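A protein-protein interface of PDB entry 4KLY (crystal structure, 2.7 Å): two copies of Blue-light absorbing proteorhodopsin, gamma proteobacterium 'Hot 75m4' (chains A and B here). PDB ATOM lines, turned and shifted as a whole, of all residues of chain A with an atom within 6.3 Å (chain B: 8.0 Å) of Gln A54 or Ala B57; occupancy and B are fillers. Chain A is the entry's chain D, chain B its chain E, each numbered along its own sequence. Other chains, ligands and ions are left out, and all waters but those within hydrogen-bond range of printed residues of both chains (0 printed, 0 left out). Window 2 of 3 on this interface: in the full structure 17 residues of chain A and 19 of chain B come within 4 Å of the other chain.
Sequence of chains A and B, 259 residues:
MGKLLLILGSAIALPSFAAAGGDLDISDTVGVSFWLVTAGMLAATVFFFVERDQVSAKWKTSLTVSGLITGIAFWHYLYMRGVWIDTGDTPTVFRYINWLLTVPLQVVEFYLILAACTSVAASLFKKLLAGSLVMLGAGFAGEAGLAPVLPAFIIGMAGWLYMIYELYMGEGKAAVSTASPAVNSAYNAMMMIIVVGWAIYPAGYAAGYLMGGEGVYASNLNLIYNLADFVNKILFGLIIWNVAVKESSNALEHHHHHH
O of Val A50 is in hydrogen-bond range of NH2 of Arg B52.
OE1 of Glu A51 is in salt-bridge range of NH2 of Arg B52 (3.4 Å).
The side-chain carboxylate of Glu A51 lies within hydrogen-bond range of the side-chain hydroxyl of Thr B61, at 2.7 Å.
OE1 of Glu A51 lies within hydrogen-bond range of OG1 of Thr B64, 2.7 Å away.
OD2 of Asp A53 lies within salt-bridge range of NH1 of Arg B52.
The side-chain amide nitrogen of Gln A54 is in hydrogen-bond range of the backbone carbonyl oxygen of Ala B57.
The side-chain amide oxygen of Gln A54 sits at hydrogen-bond distance from the side-chain hydroxyl of Thr B61, 2.9 Å away.
OE2 of Glu A51 sits close to OE1 of Gln A54, at 3.0 Å.
NE1 of Trp A241 lies within hydrogen-bond range of OE2 of Glu A51, at 3.1 Å.
O of Arg B52 sits at hydrogen-bond distance from NZ of Lys B60, 3.1 Å away.
NE of Arg B52 sits at hydrogen-bond distance from OG1 of Thr B64, 3.0 Å away.
The backbone carbonyl oxygen (O) of Val B55 sits at hydrogen-bond distance from the side-chain amino group (NZ) of Lys B60.
The backbone carbonyl oxygen (O) of Lys B60 lies within hydrogen-bond range of the side-chain hydroxyl (OG1) of Thr B64 (2.9 Å).
Among the printed residues, pairs that only touch across the chains: Gln A54 with Lys B60 (3.1 Å), Trp A241 with Thr B61 (3.4 Å) and Asp A53 with Lys B60 (3.4 Å).
Of the printed residues of chain B, Val A50 touches Arg B52 (3.4 Å).
Of the printed residues of chain B, Asp A53 touches Arg B52 and Lys B60.
Of the printed residues of chain B, Gln A54 touches Ala B57 (3.1 Å), Lys B60 (3.1 Å) and Thr B61 (2.9 Å).
Ser A56 touches none of the printed residues of chain B.
Gln B54 touches none of the printed residues of chain A.
Of chain A, only Gln A54 comes within 4 Å of Ala B57.
Of the printed residues of chain A, Lys B60 touches Asp A53 (3.4 Å) and Gln A54 (3.1 Å).
Of the printed residues of chain A, Thr B61 touches Glu A51, Gln A54 and Trp A241.
The nearest printed residue of chain B that does not touch Gln A54 is Arg B52 (4.01 Å).
The nearest printed residue of chain B that does not touch Asp A53 is Ala B57 (6.1 Å).
Hydrophobic or aromatic side chains of chain A that line the printed part of chain B: Val A50 and Trp A241.
Along chain A the printed residues that touch a printed residue of chain B span positions 50 to 241.
Of the 13 printed residues of chain B, 5 touch a printed residue of chain A.
Printed residues of chain B that touch a printed residue of chain A: Arg B52, Ala B57, Lys B60, Thr B61 and Thr B64.
Hydrophobic or aromatic side chains of chain B within 4 Å of the printed part of chain A: Ala B57.
Among the printed residues, Asp or Glu carboxylates within 4 Å of a Lys or Arg side-chain nitrogen of the other chain: Glu A51 with Arg B52 and Asp A53 with Arg B52.
Gln A54 touches Lys B60, but with the chains exchanged Lys A60 does not touch Gln B54 (15.4 Å).
Positions printed for both chains: 52, 54, 55, 56, 60 and 248.
Of the 10 pairs that touch across the chains among the printed residues, none has its exchanged pair printed and touching as well.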
ATOM      1  N   VAL A  50      15.770  10.820   0.424  1.00  0.00           N
ATOM      2  CA  VAL A  50      15.524  10.237   1.752  1.00  0.00           C
ATOM      3  C   VAL A  50      14.841  11.268   2.678  1.00  0.00           C
ATOM      4  O   VAL A  50      13.990  10.939   3.517  1.00  0.00           O
ATOM      5  CB  VAL A  50      16.846   9.773   2.400  1.00  0.00           C
ATOM      6  CG1 VAL A  50      16.677   9.445   3.882  1.00  0.00           C
ATOM      7  CG2 VAL A  50      17.459   8.582   1.651  1.00  0.00           C
ATOM      8  N   GLU A  51      15.213  12.527   2.500  1.00  0.00           N
ATOM      9  CA  GLU A  51      14.663  13.616   3.290  1.00  0.00           C
ATOM     10  C   GLU A  51      13.209  13.951   2.906  1.00  0.00           C
ATOM     11  O   GLU A  51      12.521  14.729   3.612  1.00  0.00           O
ATOM     12  CB  GLU A  51      15.571  14.849   3.186  1.00  0.00           C
ATOM     13  CG  GLU A  51      16.852  14.711   3.989  1.00  0.00           C
ATOM     14  CD  GLU A  51      16.578  14.631   5.476  1.00  0.00           C
ATOM     15  OE1 GLU A  51      16.970  13.619   6.094  1.00  0.00           O
ATOM     16  OE2 GLU A  51      15.943  15.564   6.030  1.00  0.00           O
ATOM     17  N   ARG A  52      12.714  13.330   1.837  1.00  0.00           N
ATOM     18  CA  ARG A  52      11.322  13.571   1.423  1.00  0.00           C
ATOM     19  C   ARG A  52      10.265  13.335   2.502  1.00  0.00           C
ATOM     20  O   ARG A  52       9.125  13.804   2.362  1.00  0.00           O
ATOM     21  CB  ARG A  52      10.962  12.691   0.256  1.00  0.00           C
ATOM     22  CG  ARG A  52      11.061  13.405  -1.041  1.00  0.00           C
ATOM     23  CD  ARG A  52      10.929  12.376  -2.120  1.00  0.00           C
ATOM     24  NE  ARG A  52       9.725  11.580  -1.882  1.00  0.00           N
ATOM     25  CZ  ARG A  52       8.549  11.884  -2.379  1.00  0.00           C
ATOM     26  NH1 ARG A  52       7.515  11.097  -2.154  1.00  0.00           N
ATOM     27  NH2 ARG A  52       8.425  12.980  -3.116  1.00  0.00           N
ATOM     28  N   ASP A  53      10.636  12.569   3.530  1.00  0.00           N
ATOM     29  CA  ASP A  53       9.722  12.192   4.547  1.00  0.00           C
ATOM     30  C   ASP A  53       9.793  13.167   5.756  1.00  0.00           C
ATOM     31  O   ASP A  53       9.249  12.898   6.831  1.00  0.00           O
ATOM     32  CB  ASP A  53      10.033  10.781   4.972  1.00  0.00           C
ATOM     33  CG  ASP A  53      11.279  10.718   5.720  1.00  0.00           C
ATOM     34  OD1 ASP A  53      11.955  11.767   5.646  1.00  0.00           O
ATOM     35  OD2 ASP A  53      11.586   9.668   6.354  1.00  0.00           O
ATOM     36  N   GLN A  54      10.528  14.255   5.570  1.00  0.00           N
ATOM     37  CA  GLN A  54      10.580  15.362   6.505  1.00  0.00           C
ATOM     38  C   GLN A  54      10.015  16.604   5.856  1.00  0.00           C
ATOM     39  O   GLN A  54      10.251  17.707   6.333  1.00  0.00           O
ATOM     40  CB  GLN A  54      12.015  15.670   6.874  1.00  0.00           C
ATOM     41  CG  GLN A  54      12.776  14.497   7.410  1.00  0.00           C
ATOM     42  CD  GLN A  54      13.483  14.864   8.668  1.00  0.00           C
ATOM     43  OE1 GLN A  54      14.712  14.901   8.723  1.00  0.00           O
ATOM     44  NE2 GLN A  54      12.710  15.173   9.687  1.00  0.00           N
ATOM     45  N   VAL A  55       9.309  16.431   4.741  1.00  0.00           N
ATOM     46  CA  VAL A  55       8.455  17.479   4.205  1.00  0.00           C
ATOM     47  C   VAL A  55       7.062  16.909   3.893  1.00  0.00           C
ATOM     48  O   VAL A  55       6.928  15.730   3.532  1.00  0.00           O
ATOM     49  CB  VAL A  55       9.058  18.152   2.958  1.00  0.00           C
ATOM     50  CG1 VAL A  55      10.505  18.512   3.204  1.00  0.00           C
ATOM     51  CG2 VAL A  55       8.930  17.277   1.723  1.00  0.00           C
ATOM     52  N   SER A  56       6.047  17.760   4.057  1.00  0.00           N
ATOM     53  CA  SER A  56       4.672  17.480   3.682  1.00  0.00           C
ATOM     54  C   SER A  56       4.458  17.325   2.170  1.00  0.00           C
ATOM     55  O   SER A  56       5.321  17.724   1.365  1.00  0.00           O
ATOM     56  CB  SER A  56       3.802  18.649   4.168  1.00  0.00           C
ATOM     57  OG  SER A  56       4.086  19.828   3.418  1.00  0.00           O
ATOM     58  N   LYS A  60       6.973  17.548  -1.299  1.00  0.00           N
ATOM     59  CA  LYS A  60       7.565  16.284  -1.661  1.00  0.00           C
ATOM     60  C   LYS A  60       7.979  16.143  -3.176  1.00  0.00           C
ATOM     61  O   LYS A  60       9.044  15.601  -3.527  1.00  0.00           O
ATOM     62  CB  LYS A  60       6.576  15.190  -1.277  1.00  0.00           C
ATOM     63  CG  LYS A  60       6.788  14.597   0.087  1.00  0.00           C
ATOM     64  CD  LYS A  60       5.866  13.405   0.273  1.00  0.00           C
ATOM     65  CE  LYS A  60       6.213  12.598   1.515  1.00  0.00           C
ATOM     66  NZ  LYS A  60       5.764  13.312   2.727  1.00  0.00           N
ATOM     67  N   TRP A 241      14.868  22.412   0.291  1.00  0.00           N
ATOM     68  CA  TRP A 241      14.816  21.549   1.459  1.00  0.00           C
ATOM     69  C   TRP A 241      14.639  22.320   2.770  1.00  0.00           C
ATOM     70  O   TRP A 241      13.822  21.912   3.585  1.00  0.00           O
ATOM     71  CB  TRP A 241      16.072  20.716   1.541  1.00  0.00           C
ATOM     72  CG  TRP A 241      16.163  19.849   2.785  1.00  0.00           C
ATOM     73  CD1 TRP A 241      15.573  18.628   2.982  1.00  0.00           C
ATOM     74  CD2 TRP A 241      16.922  20.116   3.979  1.00  0.00           C
ATOM     75  NE1 TRP A 241      15.910  18.130   4.228  1.00  0.00           N
ATOM     76  CE2 TRP A 241      16.739  19.025   4.850  1.00  0.00           C
ATOM     77  CE3 TRP A 241      17.724  21.176   4.397  1.00  0.00           C
ATOM     78  CZ2 TRP A 241      17.335  18.961   6.094  1.00  0.00           C
ATOM     79  CZ3 TRP A 241      18.298  21.115   5.641  1.00  0.00           C
ATOM     80  CH2 TRP A 241      18.098  20.020   6.476  1.00  0.00           C
ATOM     81  N   ALA A 244      11.287  23.859   2.973  1.00  0.00           N
ATOM     82  CA  ALA A 244      10.251  22.824   3.094  1.00  0.00           C
ATOM     83  C   ALA A 244      10.151  22.295   4.511  1.00  0.00           C
ATOM     84  O   ALA A 244       9.051  21.978   4.958  1.00  0.00           O
ATOM     85  CB  ALA A 244      10.531  21.683   2.142  1.00  0.00           C
ATOM     86  N   VAL A 245      11.299  22.223   5.200  1.00  0.00           N
ATOM     87  CA  VAL A 245      11.403  21.610   6.523  1.00  0.00           C
ATOM     88  C   VAL A 245      10.965  22.587   7.594  1.00  0.00           C
ATOM     89  O   VAL A 245      10.263  22.227   8.546  1.00  0.00           O
ATOM     90  CB  VAL A 245      12.841  21.173   6.827  1.00  0.00           C
ATOM     91  CG1 VAL A 245      13.008  20.879   8.311  1.00  0.00           C
ATOM     92  CG2 VAL A 245      13.213  19.948   6.002  1.00  0.00           C
ATOM     93  N   SER A 248       7.049  22.621   6.876  1.00  0.00           N
ATOM     94  CA  SER A 248       6.418  21.363   7.264  1.00  0.00           C
ATOM     95  C   SER A 248       6.369  21.245   8.790  1.00  0.00           C
ATOM     96  O   SER A 248       5.432  20.683   9.341  1.00  0.00           O
ATOM     97  CB  SER A 248       7.174  20.164   6.636  1.00  0.00           C
ATOM     98  OG  SER A 248       7.289  20.292   5.215  1.00  0.00           O
ATOM     99  N   SER A 249       7.379  21.799   9.457  1.00  0.00           N
ATOM    100  CA  SER A 249       7.474  21.820  10.918  1.00  0.00           C
ATOM    101  C   SER A 249       6.547  22.878  11.584  1.00  0.00           C
ATOM    102  O   SER A 249       5.911  22.610  12.613  1.00  0.00           O
ATOM    103  CB  SER A 249       8.938  22.052  11.300  1.00  0.00           C
ATOM    104  OG  SER A 249       9.126  21.895  12.687  1.00  0.00           O
ATOM    105  N   ARG B  52      16.135   5.167  10.385  1.00  0.00           N
ATOM    106  CA  ARG B  52      15.552   6.497  10.479  1.00  0.00           C
ATOM    107  C   ARG B  52      14.115   6.432  10.958  1.00  0.00           C
ATOM    108  O   ARG B  52      13.626   7.351  11.655  1.00  0.00           O
ATOM    109  CB  ARG B  52      15.605   7.193   9.134  1.00  0.00           C
ATOM    110  CG  ARG B  52      16.992   7.689   8.816  1.00  0.00           C
ATOM    111  CD  ARG B  52      17.078   8.289   7.427  1.00  0.00           C
ATOM    112  NE  ARG B  52      16.457   9.609   7.322  1.00  0.00           N
ATOM    113  CZ  ARG B  52      15.225   9.851   6.882  1.00  0.00           C
ATOM    114  NH1 ARG B  52      14.409   8.869   6.537  1.00  0.00           N
ATOM    115  NH2 ARG B  52      14.811  11.099   6.772  1.00  0.00           N
ATOM    116  N   GLN B  54      13.159   4.780  13.234  1.00  0.00           N
ATOM    117  CA  GLN B  54      13.279   4.570  14.657  1.00  0.00           C
ATOM    118  C   GLN B  54      13.585   5.857  15.370  1.00  0.00           C
ATOM    119  O   GLN B  54      13.834   5.833  16.564  1.00  0.00           O
ATOM    120  CB  GLN B  54      14.415   3.604  14.982  1.00  0.00           C
ATOM    121  CG  GLN B  54      14.125   2.147  14.682  1.00  0.00           C
ATOM    122  CD  GLN B  54      12.880   1.649  15.361  1.00  0.00           C
ATOM    123  OE1 GLN B  54      11.757   2.088  15.052  1.00  0.00           O
ATOM    124  NE2 GLN B  54      13.058   0.714  16.276  1.00  0.00           N
ATOM    125  N   VAL B  55      13.615   6.974  14.653  1.00  0.00           N
ATOM    126  CA  VAL B  55      13.773   8.259  15.303  1.00  0.00           C
ATOM    127  C   VAL B  55      12.820   9.267  14.714  1.00  0.00           C
ATOM    128  O   VAL B  55      12.323   9.065  13.617  1.00  0.00           O
ATOM    129  CB  VAL B  55      15.204   8.800  15.202  1.00  0.00           C
ATOM    130  CG1 VAL B  55      16.159   7.834  15.855  1.00  0.00           C
ATOM    131  CG2 VAL B  55      15.595   9.078  13.755  1.00  0.00           C
ATOM    132  N   SER B  56      12.597  10.359  15.446  1.00  0.00           N
ATOM    133  CA  SER B  56      11.628  11.381  15.054  1.00  0.00           C
ATOM    134  C   SER B  56      12.257  12.415  14.140  1.00  0.00           C
ATOM    135  O   SER B  56      13.465  12.555  14.098  1.00  0.00           O
ATOM    136  CB  SER B  56      11.093  12.082  16.288  1.00  0.00           C
ATOM    137  OG  SER B  56      12.167  12.629  17.006  1.00  0.00           O
ATOM    138  N   ALA B  57      11.418  13.153  13.426  1.00  0.00           N
ATOM    139  CA  ALA B  57      11.886  14.194  12.517  1.00  0.00           C
ATOM    140  C   ALA B  57      13.073  14.906  13.112  1.00  0.00           C
ATOM    141  O   ALA B  57      14.083  15.122  12.465  1.00  0.00           O
ATOM    142  CB  ALA B  57      10.774  15.191  12.232  1.00  0.00           C
ATOM    143  N   LYS B  58      12.938  15.264  14.374  1.00  0.00           N
ATOM    144  CA  LYS B  58      14.031  15.875  15.120  1.00  0.00           C
ATOM    145  C   LYS B  58      15.421  15.288  14.785  1.00  0.00           C
ATOM    146  O   LYS B  58      16.350  16.039  14.572  1.00  0.00           O
ATOM    147  CB  LYS B  58      13.736  15.743  16.614  1.00  0.00           C
ATOM    148  CG  LYS B  58      14.541  16.654  17.509  1.00  0.00           C
ATOM    149  CD  LYS B  58      14.155  16.428  18.958  1.00  0.00           C
ATOM    150  CE  LYS B  58      12.683  16.739  19.185  1.00  0.00           C
ATOM    151  NZ  LYS B  58      12.426  16.876  20.632  1.00  0.00           N
ATOM    152  N   TRP B  59      15.551  13.961  14.728  1.00  0.00           N
ATOM    153  CA  TRP B  59      16.850  13.296  14.483  1.00  0.00           C
ATOM    154  C   TRP B  59      17.089  12.728  13.081  1.00  0.00           C
ATOM    155  O   TRP B  59      18.217  12.334  12.757  1.00  0.00           O
ATOM    156  CB  TRP B  59      17.036  12.164  15.489  1.00  0.00           C
ATOM    157  CG  TRP B  59      16.918  12.654  16.856  1.00  0.00           C
ATOM    158  CD1 TRP B  59      15.781  12.749  17.599  1.00  0.00           C
ATOM    159  CD2 TRP B  59      17.973  13.187  17.654  1.00  0.00           C
ATOM    160  NE1 TRP B  59      16.072  13.281  18.834  1.00  0.00           N
ATOM    161  CE2 TRP B  59      17.409  13.574  18.886  1.00  0.00           C
ATOM    162  CE3 TRP B  59      19.339  13.370  17.450  1.00  0.00           C
ATOM    163  CZ2 TRP B  59      18.163  14.132  19.901  1.00  0.00           C
ATOM    164  CZ3 TRP B  59      20.090  13.922  18.464  1.00  0.00           C
ATOM    165  CH2 TRP B  59      19.501  14.304  19.671  1.00  0.00           C
ATOM    166  N   LYS B  60      16.048  12.682  12.263  1.00  0.00           N
ATOM    167  CA  LYS B  60      16.114  12.038  10.965  1.00  0.00           C
ATOM    168  C   LYS B  60      17.262  12.536  10.059  1.00  0.00           C
ATOM    169  O   LYS B  60      18.015  11.736   9.490  1.00  0.00           O
ATOM    170  CB  LYS B  60      14.759  12.162  10.249  1.00  0.00           C
ATOM    171  CG  LYS B  60      13.749  11.104  10.664  1.00  0.00           C
ATOM    172  CD  LYS B  60      12.550  11.147   9.749  1.00  0.00           C
ATOM    173  CE  LYS B  60      11.790   9.827   9.793  1.00  0.00           C
ATOM    174  NZ  LYS B  60      11.392   9.449  11.170  1.00  0.00           N
ATOM    175  N   THR B  61      17.377  13.852   9.922  1.00  0.00           N
ATOM    176  CA  THR B  61      18.448  14.473   9.131  1.00  0.00           C
ATOM    177  C   THR B  61      19.862  14.085   9.617  1.00  0.00           C
ATOM    178  O   THR B  61      20.759  13.783   8.804  1.00  0.00           O
ATOM    179  CB  THR B  61      18.264  16.005   9.133  1.00  0.00           C
ATOM    180  OG1 THR B  61      17.208  16.340   8.236  1.00  0.00           O
ATOM    181  CG2 THR B  61      19.508  16.738   8.680  1.00  0.00           C
ATOM    182  N   SER B  62      20.044  14.087  10.940  1.00  0.00           N
ATOM    183  CA  SER B  62      21.300  13.653  11.575  1.00  0.00           C
ATOM    184  C   SER B  62      21.761  12.278  11.124  1.00  0.00           C
ATOM    185  O   SER B  62      22.956  12.071  11.006  1.00  0.00           O
ATOM    186  CB  SER B  62      21.168  13.616  13.100  1.00  0.00           C
ATOM    187  OG  SER B  62      20.430  14.733  13.540  1.00  0.00           O
ATOM    188  N   LEU B  63      20.817  11.337  10.953  1.00  0.00           N
ATOM    189  CA  LEU B  63      21.133   9.968  10.547  1.00  0.00           C
ATOM    190  C   LEU B  63      21.459   9.890   9.042  1.00  0.00           C
ATOM    191  O   LEU B  63      22.363   9.118   8.624  1.00  0.00           O
ATOM    192  CB  LEU B  63      19.995   9.011  10.869  1.00  0.00           C
ATOM    193  CG  LEU B  63      19.751   8.517  12.304  1.00  0.00           C
ATOM    194  CD1 LEU B  63      18.988   7.190  12.289  1.00  0.00           C
ATOM    195  CD2 LEU B  63      21.029   8.360  13.089  1.00  0.00           C
ATOM    196  N   THR B  64      20.712  10.679   8.254  1.00  0.00           N
ATOM    197  CA  THR B  64      20.947  10.848   6.824  1.00  0.00           C
ATOM    198  C   THR B  64      22.376  11.311   6.582  1.00  0.00           C
ATOM    199  O   THR B  64      23.116  10.670   5.828  1.00  0.00           O
ATOM    200  CB  THR B  64      19.949  11.847   6.216  1.00  0.00           C
ATOM    201  OG1 THR B  64      18.642  11.532   6.683  1.00  0.00           O
ATOM    202  CG2 THR B  64      19.923  11.780   4.720  1.00  0.00           C
ATOM    203  N   SER B 248      13.732   9.492  21.259  1.00  0.00           N
ATOM    204  CA  SER B 248      12.563   9.306  20.393  1.00  0.00           C
ATOM    205  C   SER B 248      11.560   8.367  21.060  1.00  0.00           C
ATOM    206  O   SER B 248      10.387   8.484  20.827  1.00  0.00           O
ATOM    207  CB  SER B 248      12.965   8.803  18.981  1.00  0.00           C
ATOM    208  OG  SER B 248      13.615   9.837  18.219  1.00  0.00           O
